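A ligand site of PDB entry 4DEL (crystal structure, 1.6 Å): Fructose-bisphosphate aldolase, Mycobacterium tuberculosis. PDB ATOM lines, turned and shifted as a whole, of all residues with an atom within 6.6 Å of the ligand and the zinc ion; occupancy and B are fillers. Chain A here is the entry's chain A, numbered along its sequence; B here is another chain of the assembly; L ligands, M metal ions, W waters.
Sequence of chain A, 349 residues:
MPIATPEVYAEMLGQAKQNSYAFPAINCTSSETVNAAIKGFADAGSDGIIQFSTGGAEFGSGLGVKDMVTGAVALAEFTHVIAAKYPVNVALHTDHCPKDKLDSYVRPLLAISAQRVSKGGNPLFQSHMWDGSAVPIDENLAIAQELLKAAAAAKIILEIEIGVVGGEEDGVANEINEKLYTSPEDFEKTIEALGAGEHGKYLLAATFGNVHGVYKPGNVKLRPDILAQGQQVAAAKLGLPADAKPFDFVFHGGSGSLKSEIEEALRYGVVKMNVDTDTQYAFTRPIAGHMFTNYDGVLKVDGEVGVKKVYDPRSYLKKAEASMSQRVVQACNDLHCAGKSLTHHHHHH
NE2 of His 252 is in hydrogen-bond range of OE2 of Glu 159 (2.8 Å).
The side-chain carboxylate (OD2) of Asp 95 lies within hydrogen-bond range of the side-chain amide nitrogen (NE2) of Gln 51.
The side-chain hydroxyl (OG) of Ser 255 is in hydrogen-bond range of the backbone NH (N) of Thr 277 (3.3 Å).
N of Asp 278 sits at hydrogen-bond distance from OG of Ser 255 (2.8 Å).
OG1 of Thr 277 sits at hydrogen-bond distance from NZ of Lys 308 of chain B (2.9 Å).
The backbone carbonyl oxygen of Phe 251 is in hydrogen-bond range of the backbone NH of Asn 274, at 2.9 Å.
The backbone NH (N) of Asn 27 is in hydrogen-bond range of the backbone carbonyl oxygen (O) of Val 275, at 3.1 Å.
The backbone NH (N) of Val 275 sits at hydrogen-bond distance from the backbone carbonyl oxygen (O) of Ala 25 (2.9 Å).
Water W1 lies within hydrogen-bond range of the side-chain carboxylate (OE2) of Glu 169 (2.7 Å), an oxygen (O6) of the ligand (2.7 Å) and the side-chain amino group (NZ) of Lys 308 of chain B (3.4 Å).
Water W2 lies within hydrogen-bond range of the side-chain carboxylate (OD2) of Asp 276 (2.7 Å), a nitrogen (N1) of the ligand (2.9 Å) and the side-chain carboxylate (OE1) of Glu 169 (3.5 Å).
The zinc ion is bound by O1 of the ligand, at 2.1 Å.
NE2 of His 212 is bound to the zinc ion (2.1 Å).
ND1 of His 252 binds the zinc ion (2.1 Å).
NE2 of His 96 is bound to the zinc ion, 2.1 Å away.
O2 of the ligand binds the zinc ion (2.4 Å).
OD1 of Asn 27 touches N1 of the ligand, 3.6 Å away.
Gln 51 touches the ligand.
O of Val 211 touches O4 of the ligand, at 3.9 Å.
N of Gly 254 touches O5 of the ligand, 3.6 Å away.
CA of Val 275 touches O5 of the ligand, at 3.5 Å.
Of the 27 residues printed, 15 come within 4 Å of the ligand.
The nearest printed residue that does not touch the ligand is Lys 308 of chain B (4.3 Å).
The side-chain carboxylate (OD2) of Asp 95 sits at hydrogen-bond distance from a nitrogen (N1) of the ligand.
An oxygen (O5) of the ligand sits at hydrogen-bond distance from the backbone NH (N) of Ser 255.
OG of Ser 255 sits at hydrogen-bond distance from O5 of the ligand.
The backbone NH (N) of Thr 277 sits at hydrogen-bond distance from an oxygen (O6) of the ligand, 2.9 Å away.
The side-chain hydroxyl of Thr 277 lies within hydrogen-bond range of an oxygen (O6) of the ligand (2.6 Å).
N of Gly 253 lies close to O3 of the ligand, at 3.3 Å.
The backbone NH of Gly 213 is in hydrogen-bond range of an oxygen (O4) of the ligand (2.9 Å).
The backbone NH (N) of Asp 276 lies within hydrogen-bond range of an oxygen (O5) of the ligand (3.0 Å).
The side-chain amide oxygen (OD1) of Asn 274 lies close to an oxygen (O1) of the ligand, at 3.4 Å.
Within 4 Å of the zinc ion: His 96, His 212 and His 252.
The nearest printed residue that does not touch the zinc ion is Asn 274 (4.1 Å).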
ATOM      1  N   ALA A  25      12.952  14.332   7.981  1.00  0.00           N
ATOM      2  CA  ALA A  25      12.504  12.945   7.938  1.00  0.00           C
ATOM      3  C   ALA A  25      12.795  12.478   6.513  1.00  0.00           C
ATOM      4  O   ALA A  25      12.141  12.920   5.572  1.00  0.00           O
ATOM      5  CB  ALA A  25      11.022  12.830   8.269  1.00  0.00           C
ATOM      6  N   ASN A  27      13.108   9.913   3.479  1.00  0.00           N
ATOM      7  CA  ASN A  27      12.624   8.639   2.961  1.00  0.00           C
ATOM      8  C   ASN A  27      13.805   7.792   2.505  1.00  0.00           C
ATOM      9  O   ASN A  27      14.667   8.293   1.768  1.00  0.00           O
ATOM     10  CB  ASN A  27      11.652   8.815   1.799  1.00  0.00           C
ATOM     11  CG  ASN A  27      10.300   9.318   2.257  1.00  0.00           C
ATOM     12  OD1 ASN A  27      10.133  10.513   2.517  1.00  0.00           O
ATOM     13  ND2 ASN A  27       9.345   8.401   2.371  1.00  0.00           N
ATOM     14  N   GLN A  51      12.434   7.369   7.425  1.00  0.00           N
ATOM     15  CA  GLN A  51      11.075   6.904   7.158  1.00  0.00           C
ATOM     16  C   GLN A  51      10.962   6.028   5.920  1.00  0.00           C
ATOM     17  O   GLN A  51      11.710   6.209   4.940  1.00  0.00           O
ATOM     18  CB  GLN A  51      10.066   8.071   7.150  1.00  0.00           C
ATOM     19  CG  GLN A  51      10.243   9.114   6.065  1.00  0.00           C
ATOM     20  CD  GLN A  51       9.205  10.253   6.161  1.00  0.00           C
ATOM     21  OE1 GLN A  51       8.731  10.602   7.252  1.00  0.00           O
ATOM     22  NE2 GLN A  51       8.876  10.840   5.026  1.00  0.00           N
ATOM     23  N   ASP A  95       5.794   6.289   6.506  1.00  0.00           N
ATOM     24  CA  ASP A  95       5.149   7.390   5.797  1.00  0.00           C
ATOM     25  C   ASP A  95       3.734   6.981   5.306  1.00  0.00           C
ATOM     26  O   ASP A  95       3.278   5.865   5.580  1.00  0.00           O
ATOM     27  CB  ASP A  95       6.045   7.792   4.615  1.00  0.00           C
ATOM     28  CG  ASP A  95       5.872   9.250   4.184  1.00  0.00           C
ATOM     29  OD1 ASP A  95       5.157  10.046   4.828  1.00  0.00           O
ATOM     30  OD2 ASP A  95       6.457   9.622   3.142  1.00  0.00           O
ATOM     31  N   HIS A  96       3.058   7.909   4.610  1.00  0.00           N
ATOM     32  CA  HIS A  96       1.651   7.793   4.156  1.00  0.00           C
ATOM     33  C   HIS A  96       1.060   6.382   4.102  1.00  0.00           C
ATOM     34  O   HIS A  96       1.411   5.576   3.232  1.00  0.00           O
ATOM     35  CB  HIS A  96       1.437   8.439   2.771  1.00  0.00           C
ATOM     36  CG  HIS A  96       1.866   9.868   2.683  1.00  0.00           C
ATOM     37  ND1 HIS A  96       1.006  10.913   2.923  1.00  0.00           N
ATOM     38  CD2 HIS A  96       3.056  10.424   2.376  1.00  0.00           C
ATOM     39  CE1 HIS A  96       1.648  12.056   2.751  1.00  0.00           C
ATOM     40  NE2 HIS A  96       2.903  11.785   2.424  1.00  0.00           N
ATOM     41  N   MET A 129       2.703   6.867  10.417  1.00  0.00           N
ATOM     42  CA  MET A 129       1.755   7.792   9.824  1.00  0.00           C
ATOM     43  C   MET A 129       0.447   7.133   9.377  1.00  0.00           C
ATOM     44  O   MET A 129       0.439   6.182   8.580  1.00  0.00           O
ATOM     45  CB  MET A 129       2.351   8.545   8.624  1.00  0.00           C
ATOM     46  CG  MET A 129       1.430   9.652   8.146  1.00  0.00           C
ATOM     47  SD  MET A 129       1.902  10.454   6.611  1.00  0.00           S
ATOM     48  CE  MET A 129       0.751  11.844   6.651  1.00  0.00           C
ATOM     49  N   GLU A 159       1.496  10.033  13.577  1.00  0.00           N
ATOM     50  CA  GLU A 159       1.321  11.179  12.695  1.00  0.00           C
ATOM     51  C   GLU A 159       0.015  10.993  11.927  1.00  0.00           C
ATOM     52  O   GLU A 159      -0.282   9.900  11.437  1.00  0.00           O
ATOM     53  CB  GLU A 159       2.504  11.270  11.706  1.00  0.00           C
ATOM     54  CG  GLU A 159       2.437  12.511  10.792  1.00  0.00           C
ATOM     55  CD  GLU A 159       3.601  12.568   9.818  1.00  0.00           C
ATOM     56  OE1 GLU A 159       4.754  12.321  10.245  1.00  0.00           O
ATOM     57  OE2 GLU A 159       3.370  12.895   8.630  1.00  0.00           O
ATOM     58  N   GLU A 161      -2.851  13.149   9.043  1.00  0.00           N
ATOM     59  CA  GLU A 161      -2.889  14.208   8.039  1.00  0.00           C
ATOM     60  C   GLU A 161      -4.295  14.751   7.871  1.00  0.00           C
ATOM     61  O   GLU A 161      -5.251  13.975   7.735  1.00  0.00           O
ATOM     62  CB  GLU A 161      -2.382  13.706   6.671  1.00  0.00           C
ATOM     63  CG  GLU A 161      -2.380  14.770   5.577  1.00  0.00           C
ATOM     64  CD  GLU A 161      -1.752  14.310   4.269  1.00  0.00           C
ATOM     65  OE1 GLU A 161      -0.720  13.629   4.329  1.00  0.00           O
ATOM     66  OE2 GLU A 161      -2.292  14.656   3.185  1.00  0.00           O
ATOM     67  N   VAL A 165      -1.963  16.399   0.240  1.00  0.00           N
ATOM     68  CA  VAL A 165      -0.691  16.805  -0.365  1.00  0.00           C
ATOM     69  C   VAL A 165      -0.818  16.578  -1.867  1.00  0.00           C
ATOM     70  O   VAL A 165      -1.218  15.500  -2.285  1.00  0.00           O
ATOM     71  CB  VAL A 165       0.516  16.015   0.204  1.00  0.00           C
ATOM     72  CG1 VAL A 165       1.824  16.489  -0.428  1.00  0.00           C
ATOM     73  CG2 VAL A 165       0.590  16.159   1.723  1.00  0.00           C
ATOM     74  N   GLU A 169       2.591  10.255  -5.635  1.00  0.00           N
ATOM     75  CA  GLU A 169       3.263   9.472  -4.613  1.00  0.00           C
ATOM     76  C   GLU A 169       2.928   8.048  -4.805  1.00  0.00           C
ATOM     77  O   GLU A 169       1.865   7.589  -4.457  1.00  0.00           O
ATOM     78  CB  GLU A 169       2.992   9.949  -3.223  1.00  0.00           C
ATOM     79  CG  GLU A 169       4.074  10.781  -2.703  1.00  0.00           C
ATOM     80  CD  GLU A 169       5.417  10.459  -3.316  1.00  0.00           C
ATOM     81  OE1 GLU A 169       6.013   9.470  -2.949  1.00  0.00           O
ATOM     82  OE2 GLU A 169       5.871  11.177  -4.205  1.00  0.00           O
ATOM     83  N   VAL A 211       3.200  20.111  -2.022  1.00  0.00           N
ATOM     84  CA  VAL A 211       3.200  19.233  -3.178  1.00  0.00           C
ATOM     85  C   VAL A 211       4.417  18.300  -3.113  1.00  0.00           C
ATOM     86  O   VAL A 211       5.546  18.788  -2.946  1.00  0.00           O
ATOM     87  CB  VAL A 211       3.204  20.040  -4.515  1.00  0.00           C
ATOM     88  CG1 VAL A 211       3.282  19.114  -5.709  1.00  0.00           C
ATOM     89  CG2 VAL A 211       1.961  20.926  -4.631  1.00  0.00           C
ATOM     90  N   HIS A 212       4.182  16.998  -3.235  1.00  0.00           N
ATOM     91  CA  HIS A 212       5.261  16.009  -3.297  1.00  0.00           C
ATOM     92  C   HIS A 212       5.979  16.191  -4.634  1.00  0.00           C
ATOM     93  O   HIS A 212       5.334  16.327  -5.682  1.00  0.00           O
ATOM     94  CB  HIS A 212       4.676  14.604  -3.245  1.00  0.00           C
ATOM     95  CG  HIS A 212       4.229  14.180  -1.878  1.00  0.00           C
ATOM     96  ND1 HIS A 212       3.006  13.565  -1.653  1.00  0.00           N
ATOM     97  CD2 HIS A 212       4.835  14.262  -0.670  1.00  0.00           C
ATOM     98  CE1 HIS A 212       2.894  13.271  -0.372  1.00  0.00           C
ATOM     99  NE2 HIS A 212       3.980  13.693   0.251  1.00  0.00           N
ATOM    100  N   GLY A 213       7.308  16.176  -4.588  1.00  0.00           N
ATOM    101  CA  GLY A 213       8.124  16.283  -5.813  1.00  0.00           C
ATOM    102  C   GLY A 213       8.860  17.611  -5.910  1.00  0.00           C
ATOM    103  O   GLY A 213       8.849  18.418  -4.959  1.00  0.00           O
ATOM    104  N   VAL A 214       9.518  17.823  -7.055  1.00  0.00           N
ATOM    105  CA  VAL A 214      10.331  19.017  -7.288  1.00  0.00           C
ATOM    106  C   VAL A 214       9.957  19.603  -8.637  1.00  0.00           C
ATOM    107  O   VAL A 214      10.172  18.983  -9.677  1.00  0.00           O
ATOM    108  CB  VAL A 214      11.856  18.724  -7.189  1.00  0.00           C
ATOM    109  CG1 VAL A 214      12.706  19.905  -7.678  1.00  0.00           C
ATOM    110  CG2 VAL A 214      12.245  18.369  -5.751  1.00  0.00           C
ATOM    111  N   PHE A 251       5.734  19.123   7.911  1.00  0.00           N
ATOM    112  CA  PHE A 251       5.877  19.800   6.602  1.00  0.00           C
ATOM    113  C   PHE A 251       6.167  18.711   5.529  1.00  0.00           C
ATOM    114  O   PHE A 251       7.300  18.222   5.420  1.00  0.00           O
ATOM    115  CB  PHE A 251       7.073  20.768   6.727  1.00  0.00           C
ATOM    116  CG  PHE A 251       7.272  21.735   5.567  1.00  0.00           C
ATOM    117  CD1 PHE A 251       7.082  21.343   4.233  1.00  0.00           C
ATOM    118  CD2 PHE A 251       7.779  23.016   5.823  1.00  0.00           C
ATOM    119  CE1 PHE A 251       7.324  22.238   3.184  1.00  0.00           C
ATOM    120  CE2 PHE A 251       8.027  23.922   4.781  1.00  0.00           C
ATOM    121  CZ  PHE A 251       7.806  23.515   3.455  1.00  0.00           C
ATOM    122  N   HIS A 252       5.122  18.323   4.797  1.00  0.00           N
ATOM    123  CA  HIS A 252       5.271  17.376   3.666  1.00  0.00           C
ATOM    124  C   HIS A 252       5.711  18.081   2.384  1.00  0.00           C
ATOM    125  O   HIS A 252       5.576  19.305   2.247  1.00  0.00           O
ATOM    126  CB  HIS A 252       3.988  16.565   3.403  1.00  0.00           C
ATOM    127  CG  HIS A 252       3.773  15.455   4.390  1.00  0.00           C
ATOM    128  ND1 HIS A 252       3.834  14.126   4.054  1.00  0.00           N
ATOM    129  CD2 HIS A 252       3.483  15.496   5.718  1.00  0.00           C
ATOM    130  CE1 HIS A 252       3.612  13.384   5.133  1.00  0.00           C
ATOM    131  NE2 HIS A 252       3.391  14.202   6.152  1.00  0.00           N
ATOM    132  N   GLY A 253       6.240  17.308   1.447  1.00  0.00           N
ATOM    133  CA  GLY A 253       6.694  17.877   0.183  1.00  0.00           C
ATOM    134  C   GLY A 253       7.845  18.849   0.345  1.00  0.00           C
ATOM    135  O   GLY A 253       7.947  19.817  -0.408  1.00  0.00           O
ATOM    136  N   GLY A 254       8.727  18.587   1.322  1.00  0.00           N
ATOM    137  CA  GLY A 254       9.845  19.480   1.631  1.00  0.00           C
ATOM    138  C   GLY A 254      10.812  19.802   0.486  1.00  0.00           C
ATOM    139  O   GLY A 254      11.263  20.934   0.342  1.00  0.00           O
ATOM    140  N   SER A 255      11.078  18.809  -0.357  1.00  0.00           N
ATOM    141  CA  SER A 255      12.033  19.019  -1.456  1.00  0.00           C
ATOM    142  C   SER A 255      11.587  20.155  -2.362  1.00  0.00           C
ATOM    143  O   SER A 255      10.411  20.267  -2.665  1.00  0.00           O
ATOM    144  CB  SER A 255      12.126  17.753  -2.308  1.00  0.00           C
ATOM    145  OG  SER A 255      12.615  16.656  -1.554  1.00  0.00           O
ATOM    146  N   GLY A 256      12.542  20.966  -2.818  1.00  0.00           N
ATOM    147  CA  GLY A 256      12.253  22.022  -3.781  1.00  0.00           C
ATOM    148  C   GLY A 256      11.654  23.284  -3.185  1.00  0.00           C
ATOM    149  O   GLY A 256      11.398  24.259  -3.907  1.00  0.00           O
ATOM    150  N   ASN A 274       9.508  16.465   5.853  1.00  0.00           N
ATOM    151  CA  ASN A 274       9.760  15.267   5.059  1.00  0.00           C
ATOM    152  C   ASN A 274      10.524  15.649   3.804  1.00  0.00           C
ATOM    153  O   ASN A 274      10.151  16.614   3.117  1.00  0.00           O
ATOM    154  CB  ASN A 274       8.429  14.607   4.651  1.00  0.00           C
ATOM    155  CG  ASN A 274       7.680  13.946   5.824  1.00  0.00           C
ATOM    156  OD1 ASN A 274       6.733  13.172   5.601  1.00  0.00           O
ATOM    157  ND2 ASN A 274       8.082  14.245   7.041  1.00  0.00           N
ATOM    158  N   VAL A 275      11.578  14.889   3.504  1.00  0.00           N
ATOM    159  CA  VAL A 275      12.392  15.079   2.295  1.00  0.00           C
ATOM    160  C   VAL A 275      12.565  13.717   1.620  1.00  0.00           C
ATOM    161  O   VAL A 275      12.955  12.738   2.270  1.00  0.00           O
ATOM    162  CB  VAL A 275      13.762  15.692   2.656  1.00  0.00           C
ATOM    163  CG1 VAL A 275      14.701  15.714   1.443  1.00  0.00           C
ATOM    164  CG2 VAL A 275      13.573  17.132   3.229  1.00  0.00           C
ATOM    165  N   ASP A 276      12.231  13.649   0.335  1.00  0.00           N
ATOM    166  CA  ASP A 276      12.409  12.403  -0.431  1.00  0.00           C
ATOM    167  C   ASP A 276      12.984  12.738  -1.798  1.00  0.00           C
ATOM    168  O   ASP A 276      14.104  12.336  -2.118  1.00  0.00           O
ATOM    169  CB  ASP A 276      11.087  11.631  -0.539  1.00  0.00           C
ATOM    170  CG  ASP A 276      11.259  10.203  -1.043  1.00  0.00           C
ATOM    171  OD1 ASP A 276      12.415   9.794  -1.368  1.00  0.00           O
ATOM    172  OD2 ASP A 276      10.241   9.457  -1.078  1.00  0.00           O
ATOM    173  N   THR A 277      12.233  13.514  -2.583  1.00  0.00           N
ATOM    174  CA  THR A 277      12.627  13.784  -3.978  1.00  0.00           C
ATOM    175  C   THR A 277      14.050  14.363  -4.129  1.00  0.00           C
ATOM    176  O   THR A 277      14.823  13.920  -4.989  1.00  0.00           O
ATOM    177  CB  THR A 277      11.589  14.667  -4.691  1.00  0.00           C
ATOM    178  OG1 THR A 277      10.297  14.063  -4.589  1.00  0.00           O
ATOM    179  CG2 THR A 277      11.928  14.794  -6.177  1.00  0.00           C
ATOM    180  N   ASP A 278      14.414  15.329  -3.275  1.00  0.00           N
ATOM    181  CA  ASP A 278      15.734  15.955  -3.348  1.00  0.00           C
ATOM    182  C   ASP A 278      16.860  15.007  -2.973  1.00  0.00           C
ATOM    183  O   ASP A 278      17.921  15.056  -3.581  1.00  0.00           O
ATOM    184  CB  ASP A 278      15.811  17.223  -2.489  1.00  0.00           C
ATOM    185  CG  ASP A 278      15.377  18.480  -3.256  1.00  0.00           C
ATOM    186  OD1 ASP A 278      15.236  18.440  -4.493  1.00  0.00           O
ATOM    187  OD2 ASP A 278      15.191  19.523  -2.586  1.00  0.00           O
ATOM    188  N   GLN A 280      16.618  11.762  -3.396  1.00  0.00           N
ATOM    189  CA  GLN A 280      16.658  10.837  -4.542  1.00  0.00           C
ATOM    190  C   GLN A 280      17.553  11.411  -5.643  1.00  0.00           C
ATOM    191  O   GLN A 280      18.426  10.711  -6.182  1.00  0.00           O
ATOM    192  CB  GLN A 280      15.276  10.579  -5.102  1.00  0.00           C
ATOM    193  CG  GLN A 280      14.345   9.782  -4.158  1.00  0.00           C
ATOM    194  CD  GLN A 280      13.020   9.453  -4.805  1.00  0.00           C
ATOM    195  OE1 GLN A 280      12.354   8.481  -4.424  1.00  0.00           O
ATOM    196  NE2 GLN A 280      12.622  10.264  -5.761  1.00  0.00           N
ATOM    197  N   LYS B 308      11.486  12.898 -11.841  1.00  0.00           N
ATOM    198  CA  LYS B 308      11.560  12.060 -10.647  1.00  0.00           C
ATOM    199  C   LYS B 308      11.342  10.586 -10.925  1.00  0.00           C
ATOM    200  O   LYS B 308      12.008   9.747 -10.291  1.00  0.00           O
ATOM    201  CB  LYS B 308      10.550  12.535  -9.590  1.00  0.00           C
ATOM    202  CG  LYS B 308      10.430  11.636  -8.357  1.00  0.00           C
ATOM    203  CD  LYS B 308       9.296  12.110  -7.443  1.00  0.00           C
ATOM    204  CE  LYS B 308       9.016  11.128  -6.320  1.00  0.00           C
ATOM    205  NZ  LYS B 308       9.952  11.286  -5.179  1.00  0.00           N
HETATM  206  C1  LIG L   1       7.283  13.700   1.586  1.00  0.00           C
HETATM  207  C2  LIG L   1       8.491  14.199   0.851  1.00  0.00           C
HETATM  208  N1  LIG L   1       7.147  12.419   1.824  1.00  0.00           N
HETATM  209  O1  LIG L   1       6.045  11.995   2.517  1.00  0.00           O
HETATM  210  O2  LIG L   1       6.342  14.620   1.987  1.00  0.00           O
HETATM  211  O3  LIG L   1       8.090  15.110  -0.161  1.00  0.00           O
HETATM  212  O4  LIG L   1       8.678  16.686  -2.073  1.00  0.00           O
HETATM  213  O5  LIG L   1      10.425  15.937  -0.488  1.00  0.00           O
HETATM  214  O6  LIG L   1       9.455  14.297  -2.127  1.00  0.00           O
HETATM  215  P1  LIG L   1       9.195  15.523  -1.265  1.00  0.00           P
HETATM  216 ZN    ZN M   1       4.432  13.274   2.239  1.00  0.00          ZN
HETATM  217  O   HOH W   1       7.798  12.304  -2.750  1.00  0.00           O
HETATM  218  O   HOH W   2       7.868  10.556  -0.243  1.00  0.00           O
